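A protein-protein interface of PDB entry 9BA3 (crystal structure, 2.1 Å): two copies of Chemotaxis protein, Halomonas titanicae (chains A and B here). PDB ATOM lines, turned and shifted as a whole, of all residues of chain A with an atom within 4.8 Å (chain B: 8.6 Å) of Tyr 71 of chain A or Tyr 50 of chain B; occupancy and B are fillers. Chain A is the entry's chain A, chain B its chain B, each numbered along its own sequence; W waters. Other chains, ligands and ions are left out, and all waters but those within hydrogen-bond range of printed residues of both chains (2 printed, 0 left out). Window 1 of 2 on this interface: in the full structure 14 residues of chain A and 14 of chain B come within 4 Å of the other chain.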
ATOM      1  N   LEU A  46      23.253  -3.950  -5.894  1.00  0.00           N
ATOM      2  CA  LEU A  46      23.405  -5.378  -6.157  1.00  0.00           C
ATOM      3  C   LEU A  46      22.797  -6.210  -5.035  1.00  0.00           C
ATOM      4  O   LEU A  46      22.030  -7.148  -5.288  1.00  0.00           O
ATOM      5  CB  LEU A  46      24.882  -5.725  -6.343  1.00  0.00           C
ATOM      6  CG  LEU A  46      25.184  -7.204  -6.579  1.00  0.00           C
ATOM      7  CD1 LEU A  46      24.416  -7.685  -7.797  1.00  0.00           C
ATOM      8  CD2 LEU A  46      26.690  -7.447  -6.746  1.00  0.00           C
ATOM      9  N   SER A  49      19.140  -6.051  -5.304  1.00  0.00           N
ATOM     10  CA  SER A  49      18.646  -6.207  -6.665  1.00  0.00           C
ATOM     11  C   SER A  49      17.409  -7.090  -6.709  1.00  0.00           C
ATOM     12  O   SER A  49      17.403  -8.199  -6.168  1.00  0.00           O
ATOM     13  CB  SER A  49      19.739  -6.811  -7.546  1.00  0.00           C
ATOM     14  OG  SER A  49      19.199  -7.201  -8.793  1.00  0.00           O
ATOM     15  N   PHE A  51      16.434  -8.421  -9.457  1.00  0.00           N
ATOM     16  CA  PHE A  51      16.830  -9.516 -10.338  1.00  0.00           C
ATOM     17  C   PHE A  51      17.504 -10.631  -9.549  1.00  0.00           C
ATOM     18  O   PHE A  51      17.173 -11.811  -9.707  1.00  0.00           O
ATOM     19  CB  PHE A  51      17.752  -8.977 -11.431  1.00  0.00           C
ATOM     20  CG  PHE A  51      18.289 -10.027 -12.361  1.00  0.00           C
ATOM     21  CD1 PHE A  51      17.467 -10.639 -13.289  1.00  0.00           C
ATOM     22  CD2 PHE A  51      19.631 -10.366 -12.337  1.00  0.00           C
ATOM     23  CE1 PHE A  51      17.967 -11.588 -14.160  1.00  0.00           C
ATOM     24  CE2 PHE A  51      20.138 -11.315 -13.205  1.00  0.00           C
ATOM     25  CZ  PHE A  51      19.305 -11.925 -14.118  1.00  0.00           C
ATOM     26  N   ILE A  52      18.428 -10.267  -8.662  1.00  0.00           N
ATOM     27  CA  ILE A  52      19.085 -11.268  -7.836  1.00  0.00           C
ATOM     28  C   ILE A  52      18.076 -11.924  -6.904  1.00  0.00           C
ATOM     29  O   ILE A  52      18.086 -13.148  -6.723  1.00  0.00           O
ATOM     30  CB  ILE A  52      20.251 -10.634  -7.056  1.00  0.00           C
ATOM     31  CG1 ILE A  52      21.288 -10.065  -8.023  1.00  0.00           C
ATOM     32  CG2 ILE A  52      20.898 -11.656  -6.148  1.00  0.00           C
ATOM     33  CD1 ILE A  52      21.816 -11.086  -8.995  1.00  0.00           C
ATOM     34  N   ASP A  67      22.957 -16.124 -16.755  1.00  0.00           N
ATOM     35  CA  ASP A  67      22.349 -14.800 -16.654  1.00  0.00           C
ATOM     36  C   ASP A  67      22.936 -14.011 -15.492  1.00  0.00           C
ATOM     37  O   ASP A  67      23.207 -12.811 -15.627  1.00  0.00           O
ATOM     38  CB  ASP A  67      20.832 -14.909 -16.497  1.00  0.00           C
ATOM     39  CG  ASP A  67      20.136 -15.286 -17.781  1.00  0.00           C
ATOM     40  OD1 ASP A  67      20.790 -15.267 -18.846  1.00  0.00           O
ATOM     41  OD2 ASP A  67      18.928 -15.593 -17.726  1.00  0.00           O
ATOM     42  N   ILE A  68      23.135 -14.664 -14.344  1.00  0.00           N
ATOM     43  CA  ILE A  68      23.713 -13.978 -13.193  1.00  0.00           C
ATOM     44  C   ILE A  68      25.129 -13.515 -13.511  1.00  0.00           C
ATOM     45  O   ILE A  68      25.516 -12.383 -13.194  1.00  0.00           O
ATOM     46  CB  ILE A  68      23.685 -14.888 -11.951  1.00  0.00           C
ATOM     47  CG1 ILE A  68      22.269 -15.406 -11.679  1.00  0.00           C
ATOM     48  CG2 ILE A  68      24.204 -14.131 -10.742  1.00  0.00           C
ATOM     49  CD1 ILE A  68      21.251 -14.318 -11.434  1.00  0.00           C
ATOM     50  N   ALA A  69      25.918 -14.380 -14.150  1.00  0.00           N
ATOM     51  CA  ALA A  69      27.289 -14.023 -14.493  1.00  0.00           C
ATOM     52  C   ALA A  69      27.332 -12.881 -15.503  1.00  0.00           C
ATOM     53  O   ALA A  69      28.207 -12.012 -15.426  1.00  0.00           O
ATOM     54  CB  ALA A  69      28.026 -15.249 -15.033  1.00  0.00           C
ATOM     55  N   ALA A  70      26.419 -12.883 -16.479  1.00  0.00           N
ATOM     56  CA  ALA A  70      26.374 -11.785 -17.443  1.00  0.00           C
ATOM     57  C   ALA A  70      25.883 -10.495 -16.792  1.00  0.00           C
ATOM     58  O   ALA A  70      26.341  -9.400 -17.139  1.00  0.00           O
ATOM     59  CB  ALA A  70      25.497 -12.160 -18.638  1.00  0.00           C
ATOM     60  N   TYR A  71      24.951 -10.608 -15.845  1.00  0.00           N
ATOM     61  CA  TYR A  71      24.496  -9.440 -15.098  1.00  0.00           C
ATOM     62  C   TYR A  71      25.650  -8.803 -14.331  1.00  0.00           C
ATOM     63  O   TYR A  71      25.859  -7.586 -14.399  1.00  0.00           O
ATOM     64  CB  TYR A  71      23.368  -9.857 -14.152  1.00  0.00           C
ATOM     65  CG  TYR A  71      22.674  -8.733 -13.416  1.00  0.00           C
ATOM     66  CD1 TYR A  71      21.643  -8.014 -14.007  1.00  0.00           C
ATOM     67  CD2 TYR A  71      23.031  -8.416 -12.110  1.00  0.00           C
ATOM     68  CE1 TYR A  71      20.999  -6.997 -13.324  1.00  0.00           C
ATOM     69  CE2 TYR A  71      22.394  -7.404 -11.421  1.00  0.00           C
ATOM     70  CZ  TYR A  71      21.379  -6.697 -12.032  1.00  0.00           C
ATOM     71  OH  TYR A  71      20.739  -5.688 -11.348  1.00  0.00           O
ATOM     72  N   LEU A  72      26.436  -9.623 -13.628  1.00  0.00           N
ATOM     73  CA  LEU A  72      27.562  -9.099 -12.861  1.00  0.00           C
ATOM     74  C   LEU A  72      28.636  -8.506 -13.766  1.00  0.00           C
ATOM     75  O   LEU A  72      29.273  -7.513 -13.395  1.00  0.00           O
ATOM     76  CB  LEU A  72      28.155 -10.204 -11.984  1.00  0.00           C
ATOM     77  CG  LEU A  72      27.254 -10.751 -10.874  1.00  0.00           C
ATOM     78  CD1 LEU A  72      27.862 -11.989 -10.221  1.00  0.00           C
ATOM     79  CD2 LEU A  72      26.986  -9.670  -9.834  1.00  0.00           C
ATOM     80  N   ALA A  73      28.843  -9.084 -14.952  1.00  0.00           N
ATOM     81  CA  ALA A  73      29.877  -8.578 -15.850  1.00  0.00           C
ATOM     82  C   ALA A  73      29.613  -7.133 -16.254  1.00  0.00           C
ATOM     83  O   ALA A  73      30.556  -6.348 -16.415  1.00  0.00           O
ATOM     84  CB  ALA A  73      29.987  -9.467 -17.089  1.00  0.00           C
ATOM     85  N   ARG A  74      28.339  -6.759 -16.428  1.00  0.00           N
ATOM     86  CA  ARG A  74      28.016  -5.359 -16.701  1.00  0.00           C
ATOM     87  C   ARG A  74      28.443  -4.461 -15.553  1.00  0.00           C
ATOM     88  O   ARG A  74      29.010  -3.384 -15.774  1.00  0.00           O
ATOM     89  CB  ARG A  74      26.517  -5.180 -16.954  1.00  0.00           C
ATOM     90  CG  ARG A  74      25.978  -5.902 -18.154  1.00  0.00           C
ATOM     91  CD  ARG A  74      26.551  -5.298 -19.415  1.00  0.00           C
ATOM     92  NE  ARG A  74      26.144  -6.037 -20.603  1.00  0.00           N
ATOM     93  CZ  ARG A  74      25.097  -5.738 -21.359  1.00  0.00           C
ATOM     94  NH1 ARG A  74      24.823  -6.425 -22.455  1.00  0.00           N
ATOM     95  NH2 ARG A  74      24.317  -4.716 -21.016  1.00  0.00           N
ATOM     96  N   LEU A  75      28.160  -4.881 -14.318  1.00  0.00           N
ATOM     97  CA  LEU A  75      28.523  -4.073 -13.160  1.00  0.00           C
ATOM     98  C   LEU A  75      30.034  -3.947 -13.024  1.00  0.00           C
ATOM     99  O   LEU A  75      30.548  -2.877 -12.677  1.00  0.00           O
ATOM    100  CB  LEU A  75      27.935  -4.675 -11.886  1.00  0.00           C
ATOM    101  CG  LEU A  75      26.416  -4.608 -11.731  1.00  0.00           C
ATOM    102  CD1 LEU A  75      25.999  -5.198 -10.391  1.00  0.00           C
ATOM    103  CD2 LEU A  75      25.920  -3.179 -11.885  1.00  0.00           C
ATOM    104  N   GLU B  44      23.751   5.026 -14.866  1.00  0.00           N
ATOM    105  CA  GLU B  44      24.620   4.274 -15.770  1.00  0.00           C
ATOM    106  C   GLU B  44      24.334   2.777 -15.705  1.00  0.00           C
ATOM    107  O   GLU B  44      24.236   2.114 -16.745  1.00  0.00           O
ATOM    108  CB  GLU B  44      26.091   4.548 -15.446  1.00  0.00           C
ATOM    109  CG  GLU B  44      27.070   3.742 -16.291  1.00  0.00           C
ATOM    110  CD  GLU B  44      28.517   4.049 -15.962  1.00  0.00           C
ATOM    111  OE1 GLU B  44      28.764   4.966 -15.150  1.00  0.00           O
ATOM    112  OE2 GLU B  44      29.410   3.377 -16.520  1.00  0.00           O
ATOM    113  N   SER B  45      24.180   2.226 -14.497  1.00  0.00           N
ATOM    114  CA  SER B  45      23.907   0.797 -14.375  1.00  0.00           C
ATOM    115  C   SER B  45      22.526   0.436 -14.905  1.00  0.00           C
ATOM    116  O   SER B  45      22.342  -0.657 -15.450  1.00  0.00           O
ATOM    117  CB  SER B  45      24.052   0.349 -12.920  1.00  0.00           C
ATOM    118  OG  SER B  45      23.124   1.024 -12.093  1.00  0.00           O
ATOM    119  N   LEU B  46      21.549   1.337 -14.771  1.00  0.00           N
ATOM    120  CA  LEU B  46      20.223   1.077 -15.323  1.00  0.00           C
ATOM    121  C   LEU B  46      20.249   1.086 -16.849  1.00  0.00           C
ATOM    122  O   LEU B  46      19.705   0.182 -17.497  1.00  0.00           O
ATOM    123  CB  LEU B  46      19.224   2.108 -14.791  1.00  0.00           C
ATOM    124  CG  LEU B  46      17.801   2.013 -15.346  1.00  0.00           C
ATOM    125  CD1 LEU B  46      17.224   0.629 -15.099  1.00  0.00           C
ATOM    126  CD2 LEU B  46      16.907   3.111 -14.749  1.00  0.00           C
ATOM    127  N   ALA B  47      20.892   2.094 -17.444  1.00  0.00           N
ATOM    128  CA  ALA B  47      20.966   2.171 -18.900  1.00  0.00           C
ATOM    129  C   ALA B  47      21.700   0.969 -19.485  1.00  0.00           C
ATOM    130  O   ALA B  47      21.364   0.500 -20.581  1.00  0.00           O
ATOM    131  CB  ALA B  47      21.639   3.478 -19.322  1.00  0.00           C
ATOM    132  N   ASN B  48      22.713   0.466 -18.781  1.00  0.00           N
ATOM    133  CA  ASN B  48      23.493  -0.686 -19.218  1.00  0.00           C
ATOM    134  C   ASN B  48      23.036  -1.995 -18.582  1.00  0.00           C
ATOM    135  O   ASN B  48      23.770  -2.987 -18.642  1.00  0.00           O
ATOM    136  CB  ASN B  48      24.979  -0.460 -18.929  1.00  0.00           C
ATOM    137  CG  ASN B  48      25.587   0.589 -19.825  1.00  0.00           C
ATOM    138  OD1 ASN B  48      25.829   0.340 -21.008  1.00  0.00           O
ATOM    139  ND2 ASN B  48      25.844   1.768 -19.271  1.00  0.00           N
ATOM    140  N   SER B  49      21.860  -2.017 -17.965  1.00  0.00           N
ATOM    141  CA  SER B  49      21.407  -3.207 -17.257  1.00  0.00           C
ATOM    142  C   SER B  49      21.255  -4.395 -18.198  1.00  0.00           C
ATOM    143  O   SER B  49      20.599  -4.299 -19.240  1.00  0.00           O
ATOM    144  CB  SER B  49      20.079  -2.928 -16.562  1.00  0.00           C
ATOM    145  OG  SER B  49      19.521  -4.133 -16.078  1.00  0.00           O
ATOM    146  N   TYR B  50      21.874  -5.519 -17.828  1.00  0.00           N
ATOM    147  CA  TYR B  50      21.631  -6.768 -18.543  1.00  0.00           C
ATOM    148  C   TYR B  50      20.177  -7.204 -18.428  1.00  0.00           C
ATOM    149  O   TYR B  50      19.612  -7.748 -19.383  1.00  0.00           O
ATOM    150  CB  TYR B  50      22.548  -7.866 -18.003  1.00  0.00           C
ATOM    151  CG  TYR B  50      22.439  -9.171 -18.755  1.00  0.00           C
ATOM    152  CD1 TYR B  50      23.062  -9.346 -19.985  1.00  0.00           C
ATOM    153  CD2 TYR B  50      21.695 -10.223 -18.240  1.00  0.00           C
ATOM    154  CE1 TYR B  50      22.955 -10.547 -20.676  1.00  0.00           C
ATOM    155  CE2 TYR B  50      21.580 -11.422 -18.919  1.00  0.00           C
ATOM    156  CZ  TYR B  50      22.210 -11.579 -20.135  1.00  0.00           C
ATOM    157  OH  TYR B  50      22.091 -12.773 -20.805  1.00  0.00           O
ATOM    158  N   PHE B  51      19.554  -6.954 -17.277  1.00  0.00           N
ATOM    159  CA  PHE B  51      18.159  -7.321 -17.080  1.00  0.00           C
ATOM    160  C   PHE B  51      17.254  -6.549 -18.031  1.00  0.00           C
ATOM    161  O   PHE B  51      16.374  -7.129 -18.678  1.00  0.00           O
ATOM    162  CB  PHE B  51      17.775  -7.072 -15.618  1.00  0.00           C
ATOM    163  CG  PHE B  51      16.326  -7.330 -15.307  1.00  0.00           C
ATOM    164  CD1 PHE B  51      15.826  -8.619 -15.280  1.00  0.00           C
ATOM    165  CD2 PHE B  51      15.475  -6.278 -14.999  1.00  0.00           C
ATOM    166  CE1 PHE B  51      14.498  -8.856 -14.981  1.00  0.00           C
ATOM    167  CE2 PHE B  51      14.143  -6.507 -14.694  1.00  0.00           C
ATOM    168  CZ  PHE B  51      13.655  -7.800 -14.688  1.00  0.00           C
ATOM    169  N   ILE B  52      17.476  -5.238 -18.149  1.00  0.00           N
ATOM    170  CA  ILE B  52      16.679  -4.432 -19.065  1.00  0.00           C
ATOM    171  C   ILE B  52      16.955  -4.840 -20.506  1.00  0.00           C
ATOM    172  O   ILE B  52      16.033  -4.949 -21.322  1.00  0.00           O
ATOM    173  CB  ILE B  52      16.952  -2.932 -18.838  1.00  0.00           C
ATOM    174  CG1 ILE B  52      16.593  -2.536 -17.403  1.00  0.00           C
ATOM    175  CG2 ILE B  52      16.195  -2.084 -19.863  1.00  0.00           C
ATOM    176  CD1 ILE B  52      15.169  -2.866 -17.012  1.00  0.00           C
ATOM    177  N   GLU B  53      18.229  -5.083 -20.838  1.00  0.00           N
ATOM    178  CA  GLU B  53      18.576  -5.463 -22.204  1.00  0.00           C
ATOM    179  C   GLU B  53      17.898  -6.768 -22.602  1.00  0.00           C
ATOM    180  O   GLU B  53      17.382  -6.887 -23.719  1.00  0.00           O
ATOM    181  CB  GLU B  53      20.094  -5.576 -22.357  1.00  0.00           C
ATOM    182  CG  GLU B  53      20.525  -6.126 -23.706  1.00  0.00           C
ATOM    183  CD  GLU B  53      22.021  -6.040 -23.930  1.00  0.00           C
ATOM    184  OE1 GLU B  53      22.664  -5.149 -23.339  1.00  0.00           O
ATOM    185  OE2 GLU B  53      22.555  -6.864 -24.702  1.00  0.00           O
ATOM    186  N   GLN B  54      17.894  -7.758 -21.703  1.00  0.00           N
ATOM    187  CA  GLN B  54      17.165  -8.996 -21.961  1.00  0.00           C
ATOM    188  C   GLN B  54      15.717  -8.707 -22.332  1.00  0.00           C
ATOM    189  O   GLN B  54      15.189  -9.256 -23.303  1.00  0.00           O
ATOM    190  CB  GLN B  54      17.214  -9.910 -20.734  1.00  0.00           C
ATOM    191  CG  GLN B  54      18.319 -10.946 -20.731  1.00  0.00           C
ATOM    192  CD  GLN B  54      18.143 -11.962 -19.610  1.00  0.00           C
ATOM    193  OE1 GLN B  54      17.409 -11.721 -18.647  1.00  0.00           O
ATOM    194  NE2 GLN B  54      18.808 -13.104 -19.734  1.00  0.00           N
ATOM    195  N   TRP B  55      15.061  -7.835 -21.563  1.00  0.00           N
ATOM    196  CA  TRP B  55      13.670  -7.501 -21.843  1.00  0.00           C
ATOM    197  C   TRP B  55      13.528  -6.869 -23.224  1.00  0.00           C
ATOM    198  O   TRP B  55      12.613  -7.218 -23.980  1.00  0.00           O
ATOM    199  CB  TRP B  55      13.139  -6.570 -20.752  1.00  0.00           C
ATOM    200  CG  TRP B  55      11.708  -6.136 -20.913  1.00  0.00           C
ATOM    201  CD1 TRP B  55      10.618  -6.938 -21.115  1.00  0.00           C
ATOM    202  CD2 TRP B  55      11.211  -4.793 -20.852  1.00  0.00           C
ATOM    203  NE1 TRP B  55       9.476  -6.172 -21.199  1.00  0.00           N
ATOM    204  CE2 TRP B  55       9.814  -4.852 -21.041  1.00  0.00           C
ATOM    205  CE3 TRP B  55      11.814  -3.544 -20.666  1.00  0.00           C
ATOM    206  CZ2 TRP B  55       9.011  -3.711 -21.048  1.00  0.00           C
ATOM    207  CZ3 TRP B  55      11.014  -2.412 -20.673  1.00  0.00           C
ATOM    208  CH2 TRP B  55       9.629  -2.505 -20.862  1.00  0.00           C
ATOM    209  N   VAL B  56      14.457  -5.978 -23.590  1.00  0.00           N
ATOM    210  CA  VAL B  56      14.435  -5.356 -24.914  1.00  0.00           C
ATOM    211  C   VAL B  56      14.678  -6.393 -26.008  1.00  0.00           C
ATOM    212  O   VAL B  56      13.999  -6.387 -27.043  1.00  0.00           O
ATOM    213  CB  VAL B  56      15.461  -4.211 -24.982  1.00  0.00           C
ATOM    214  CG1 VAL B  56      15.478  -3.596 -26.366  1.00  0.00           C
ATOM    215  CG2 VAL B  56      15.151  -3.148 -23.933  1.00  0.00           C
ATOM    216  N   ARG B  57      15.651  -7.291 -25.807  1.00  0.00           N
ATOM    217  CA  ARG B  57      15.943  -8.313 -26.811  1.00  0.00           C
ATOM    218  C   ARG B  57      14.753  -9.233 -27.044  1.00  0.00           C
ATOM    219  O   ARG B  57      14.581  -9.758 -28.150  1.00  0.00           O
ATOM    220  CB  ARG B  57      17.141  -9.162 -26.383  1.00  0.00           C
ATOM    221  CG  ARG B  57      18.474  -8.452 -26.236  1.00  0.00           C
ATOM    222  CD  ARG B  57      19.003  -7.963 -27.552  1.00  0.00           C
ATOM    223  NE  ARG B  57      20.394  -7.542 -27.440  1.00  0.00           N
ATOM    224  CZ  ARG B  57      21.109  -7.059 -28.447  1.00  0.00           C
ATOM    225  NH1 ARG B  57      20.591  -6.922 -29.655  1.00  0.00           N
ATOM    226  NH2 ARG B  57      22.374  -6.703 -28.235  1.00  0.00           N
ATOM    227  N   GLU B  58      13.941  -9.462 -26.014  1.00  0.00           N
ATOM    228  CA  GLU B  58      12.761 -10.309 -26.124  1.00  0.00           C
ATOM    229  C   GLU B  58      11.595  -9.620 -26.818  1.00  0.00           C
ATOM    230  O   GLU B  58      10.547 -10.249 -26.992  1.00  0.00           O
ATOM    231  CB  GLU B  58      12.328 -10.776 -24.731  1.00  0.00           C
ATOM    232  CG  GLU B  58      13.289 -11.761 -24.082  1.00  0.00           C
ATOM    233  CD  GLU B  58      13.067 -11.917 -22.583  1.00  0.00           C
ATOM    234  OE1 GLU B  58      12.072 -11.374 -22.049  1.00  0.00           O
ATOM    235  OE2 GLU B  58      13.901 -12.583 -21.936  1.00  0.00           O
ATOM    236  N   ARG B  64       6.057  -8.978 -18.914  1.00  0.00           N
ATOM    237  CA  ARG B  64       7.149  -8.780 -17.973  1.00  0.00           C
ATOM    238  C   ARG B  64       7.231  -7.351 -17.450  1.00  0.00           C
ATOM    239  O   ARG B  64       8.175  -7.024 -16.724  1.00  0.00           O
ATOM    240  CB  ARG B  64       8.465  -9.184 -18.631  1.00  0.00           C
ATOM    241  CG  ARG B  64       8.442 -10.622 -19.132  1.00  0.00           C
ATOM    242  CD  ARG B  64       9.832 -11.176 -19.327  1.00  0.00           C
ATOM    243  NE  ARG B  64      10.697 -10.878 -18.193  1.00  0.00           N
ATOM    244  CZ  ARG B  64      11.867 -10.267 -18.293  1.00  0.00           C
ATOM    245  NH1 ARG B  64      12.355  -9.898 -19.466  1.00  0.00           N
ATOM    246  NH2 ARG B  64      12.574 -10.034 -17.190  1.00  0.00           N
ATOM    247  N   ILE B  68       9.658  -5.336 -14.657  1.00  0.00           N
ATOM    248  CA  ILE B  68      10.419  -4.118 -14.928  1.00  0.00           C
ATOM    249  C   ILE B  68      10.070  -3.040 -13.911  1.00  0.00           C
ATOM    250  O   ILE B  68      10.953  -2.348 -13.390  1.00  0.00           O
ATOM    251  CB  ILE B  68      10.170  -3.636 -16.370  1.00  0.00           C
ATOM    252  CG1 ILE B  68      10.461  -4.758 -17.372  1.00  0.00           C
ATOM    253  CG2 ILE B  68      11.010  -2.396 -16.673  1.00  0.00           C
ATOM    254  CD1 ILE B  68      11.879  -5.291 -17.316  1.00  0.00           C
ATOM    255  N   TYR B  71      11.617  -3.929 -10.592  1.00  0.00           N
ATOM    256  CA  TYR B  71      13.047  -3.658 -10.651  1.00  0.00           C
ATOM    257  C   TYR B  71      13.318  -2.171 -10.453  1.00  0.00           C
ATOM    258  O   TYR B  71      14.188  -1.786  -9.664  1.00  0.00           O
ATOM    259  CB  TYR B  71      13.597  -4.147 -11.989  1.00  0.00           C
ATOM    260  CG  TYR B  71      15.102  -4.126 -12.127  1.00  0.00           C
ATOM    261  CD1 TYR B  71      15.874  -5.177 -11.655  1.00  0.00           C
ATOM    262  CD2 TYR B  71      15.748  -3.073 -12.770  1.00  0.00           C
ATOM    263  CE1 TYR B  71      17.254  -5.173 -11.794  1.00  0.00           C
ATOM    264  CE2 TYR B  71      17.129  -3.061 -12.919  1.00  0.00           C
ATOM    265  CZ  TYR B  71      17.876  -4.115 -12.427  1.00  0.00           C
ATOM    266  OH  TYR B  71      19.246  -4.128 -12.562  1.00  0.00           O
ATOM    267  N   LEU B  75      15.109   0.197  -7.194  1.00  0.00           N
ATOM    268  CA  LEU B  75      16.125   1.240  -7.339  1.00  0.00           C
ATOM    269  C   LEU B  75      15.669   2.552  -6.717  1.00  0.00           C
ATOM    270  O   LEU B  75      16.474   3.285  -6.131  1.00  0.00           O
ATOM    271  CB  LEU B  75      16.470   1.457  -8.811  1.00  0.00           C
ATOM    272  CG  LEU B  75      17.255   0.367  -9.536  1.00  0.00           C
ATOM    273  CD1 LEU B  75      17.534   0.808 -10.958  1.00  0.00           C
ATOM    274  CD2 LEU B  75      18.560   0.076  -8.810  1.00  0.00           C
ATOM    275  N   VAL B 153      25.613  -0.427 -25.690  1.00  0.00           N
ATOM    276  CA  VAL B 153      25.084  -1.154 -26.839  1.00  0.00           C
ATOM    277  C   VAL B 153      24.165  -0.248 -27.649  1.00  0.00           C
ATOM    278  O   VAL B 153      23.306   0.450 -27.095  1.00  0.00           O
ATOM    279  CB  VAL B 153      24.342  -2.415 -26.371  1.00  0.00           C
ATOM    280  CG1 VAL B 153      23.663  -3.115 -27.542  1.00  0.00           C
ATOM    281  CG2 VAL B 153      25.296  -3.357 -25.660  1.00  0.00           C
ATOM    282  N   LEU B 161      20.577   1.324 -27.574  1.00  0.00           N
ATOM    283  CA  LEU B 161      19.542   0.348 -27.263  1.00  0.00           C
ATOM    284  C   LEU B 161      18.655   0.840 -26.126  1.00  0.00           C
ATOM    285  O   LEU B 161      17.430   0.671 -26.166  1.00  0.00           O
ATOM    286  CB  LEU B 161      20.181  -0.993 -26.911  1.00  0.00           C
ATOM    287  CG  LEU B 161      19.211  -2.171 -26.826  1.00  0.00           C
ATOM    288  CD1 LEU B 161      18.625  -2.486 -28.194  1.00  0.00           C
ATOM    289  CD2 LEU B 161      19.900  -3.391 -26.244  1.00  0.00           C
ATOM    290  N   VAL B 162      19.255   1.472 -25.119  1.00  0.00           N
ATOM    291  CA  VAL B 162      18.537   1.966 -23.948  1.00  0.00           C
ATOM    292  C   VAL B 162      19.100   3.325 -23.561  1.00  0.00           C
ATOM    293  O   VAL B 162      20.320   3.492 -23.451  1.00  0.00           O
ATOM    294  CB  VAL B 162      18.644   0.998 -22.752  1.00  0.00           C
ATOM    295  CG1 VAL B 162      18.062   1.634 -21.501  1.00  0.00           C
ATOM    296  CG2 VAL B 162      17.930  -0.315 -23.049  1.00  0.00           C
HETATM  297  O   HOH W   1      23.528  -5.468 -15.348  1.00  0.00           O
HETATM  298  O   HOH W   2      22.344  -2.697 -23.000  1.00  0.00           O
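Phe 51 of chain A touches its own counterpart, Phe 51 of chain B.
Phe 51 of chain A touches Tyr 71 of chain B, and with the chains exchanged Tyr 71 of chain A touches Phe 51 of chain B.
Tyr 71 of chain A touches its own counterpart, Tyr 71 of chain B.
Positions printed for both chains: 46, 49, 51, 52, 68, 71 and 75.
Of the 11 pairs that touch across the chains among the printed residues, 4 have their exchanged pair printed and touching as well.
Water W2 bridges OE1 of Glu 53 of chain B and NH2 of Arg 74 of chain A.
Water W1 lies within hydrogen-bond range of N of Tyr 50 of chain B (3.0 Å) and O of Tyr 71 of chain A (3.3 Å).
Phe 51 of chain A touches Phe 51 of chain B (CD1 to CD1, 3.3 Å).
CE1 of Tyr 71 of chain B touches CB of Phe 51 of chain A, at 3.9 Å.
Tyr 50 of chain B touches Ala 70 of chain A.
Tyr 50 of chain B touches Tyr 71 of chain A (CB to CA, 3.8 Å).
CE1 of Tyr 71 of chain A touches CB of Phe 51 of chain B, 3.96 Å away.
Arg 74 of chain A touches Tyr 50 of chain B (CG to CB, 3.96 Å).
The side-chain carboxylate (OD1) of Asp 67 of chain A is in hydrogen-bond range of the side-chain amide nitrogen (NE2) of Gln 54 of chain B, 3.1 Å away.
OE1 of Glu 53 of chain B is in salt-bridge range of NH1 of Arg 74 of chain A (2.7 Å).
NH2 of Arg 74 of chain A lies within hydrogen-bond range of O of Asn 48 of chain B (3.0 Å).
The side-chain hydroxyl (OH) of Tyr 71 of chain A is in hydrogen-bond range of the side-chain hydroxyl (OH) of Tyr 71 of chain B, at 2.5 Å.
The side-chain carboxylate (OD1) of Asp 67 of chain A lies within hydrogen-bond range of the side-chain hydroxyl (OH) of Tyr 50 of chain B, at 3.4 Å.
The backbone NH (N) of Phe 51 of chain A is in hydrogen-bond range of the side-chain hydroxyl (OG) of Ser 49 of chain A.
The side-chain carboxylate of Glu 53 of chain B is in salt-bridge range of the guanidinium group of Arg 57 of chain B (3.5 Å).
The side-chain amide nitrogen (ND2) of Asn 48 of chain B sits at hydrogen-bond distance from the backbone carbonyl oxygen (O) of Glu 44 of chain B.
The side-chain hydroxyl (OG) of Ser 49 of chain B is in hydrogen-bond range of the backbone NH (N) of Phe 51 of chain B (3.1 Å).
The side-chain hydroxyl of Ser 49 of chain A sits at hydrogen-bond distance from the side-chain hydroxyl of Tyr 71 of chain A (3.3 Å).
OH of Tyr 50 of chain B sits close to NE2 of Gln 54 of chain B (3.5 Å).
Hydrophobic or aromatic side chains of chain A within 4 Å of the printed part of chain B: Phe 51, Ala 70 and Tyr 71.
Among the printed residues, 11 pairs touch across the chains.
Among the printed residues, Asp or Glu carboxylates within 4 Å of a Lys or Arg side-chain nitrogen of the other chain: Arg 74 of chain A with Glu 53 of chain B (2.7 Å).
Of chain B, only Tyr 50 (3.8 Å), Phe 51 (3.96 Å) and Tyr 71 (2.5 Å) come within 4 Å of Tyr 71 of chain A.
Tyr 50 of chain B touches just these residues of chain A: Asp 67, Ala 70, Tyr 71 and Arg 74.
Of chain B, only Tyr 50 (3.6 Å) comes within 4 Å of Ala 70 of chain A.
Printed residues of chain A within 4 Å of Tyr 71 of chain B: Phe 51 (3.9 Å) and Tyr 71 (2.5 Å).
Of the printed residues of chain B, Arg 74 of chain A touches Asn 48 (3.0 Å), Tyr 50 (3.96 Å) and Glu 53 (2.7 Å).
Ile 52 of chain B touches none of the printed residues of chain A.
Arg 57 of chain B touches none of the printed residues of chain A.
The nearest residue of chain B that does not touch Tyr 71 of chain A is Ser 49 of chain B (4.2 Å).
The nearest printed residue of chain A that does not touch Tyr 50 of chain B is Phe 51 of chain A (5.1 Å).
The nearest printed residue of chain B that does not touch Arg 74 of chain A is Ser 49 of chain B (4.1 Å).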
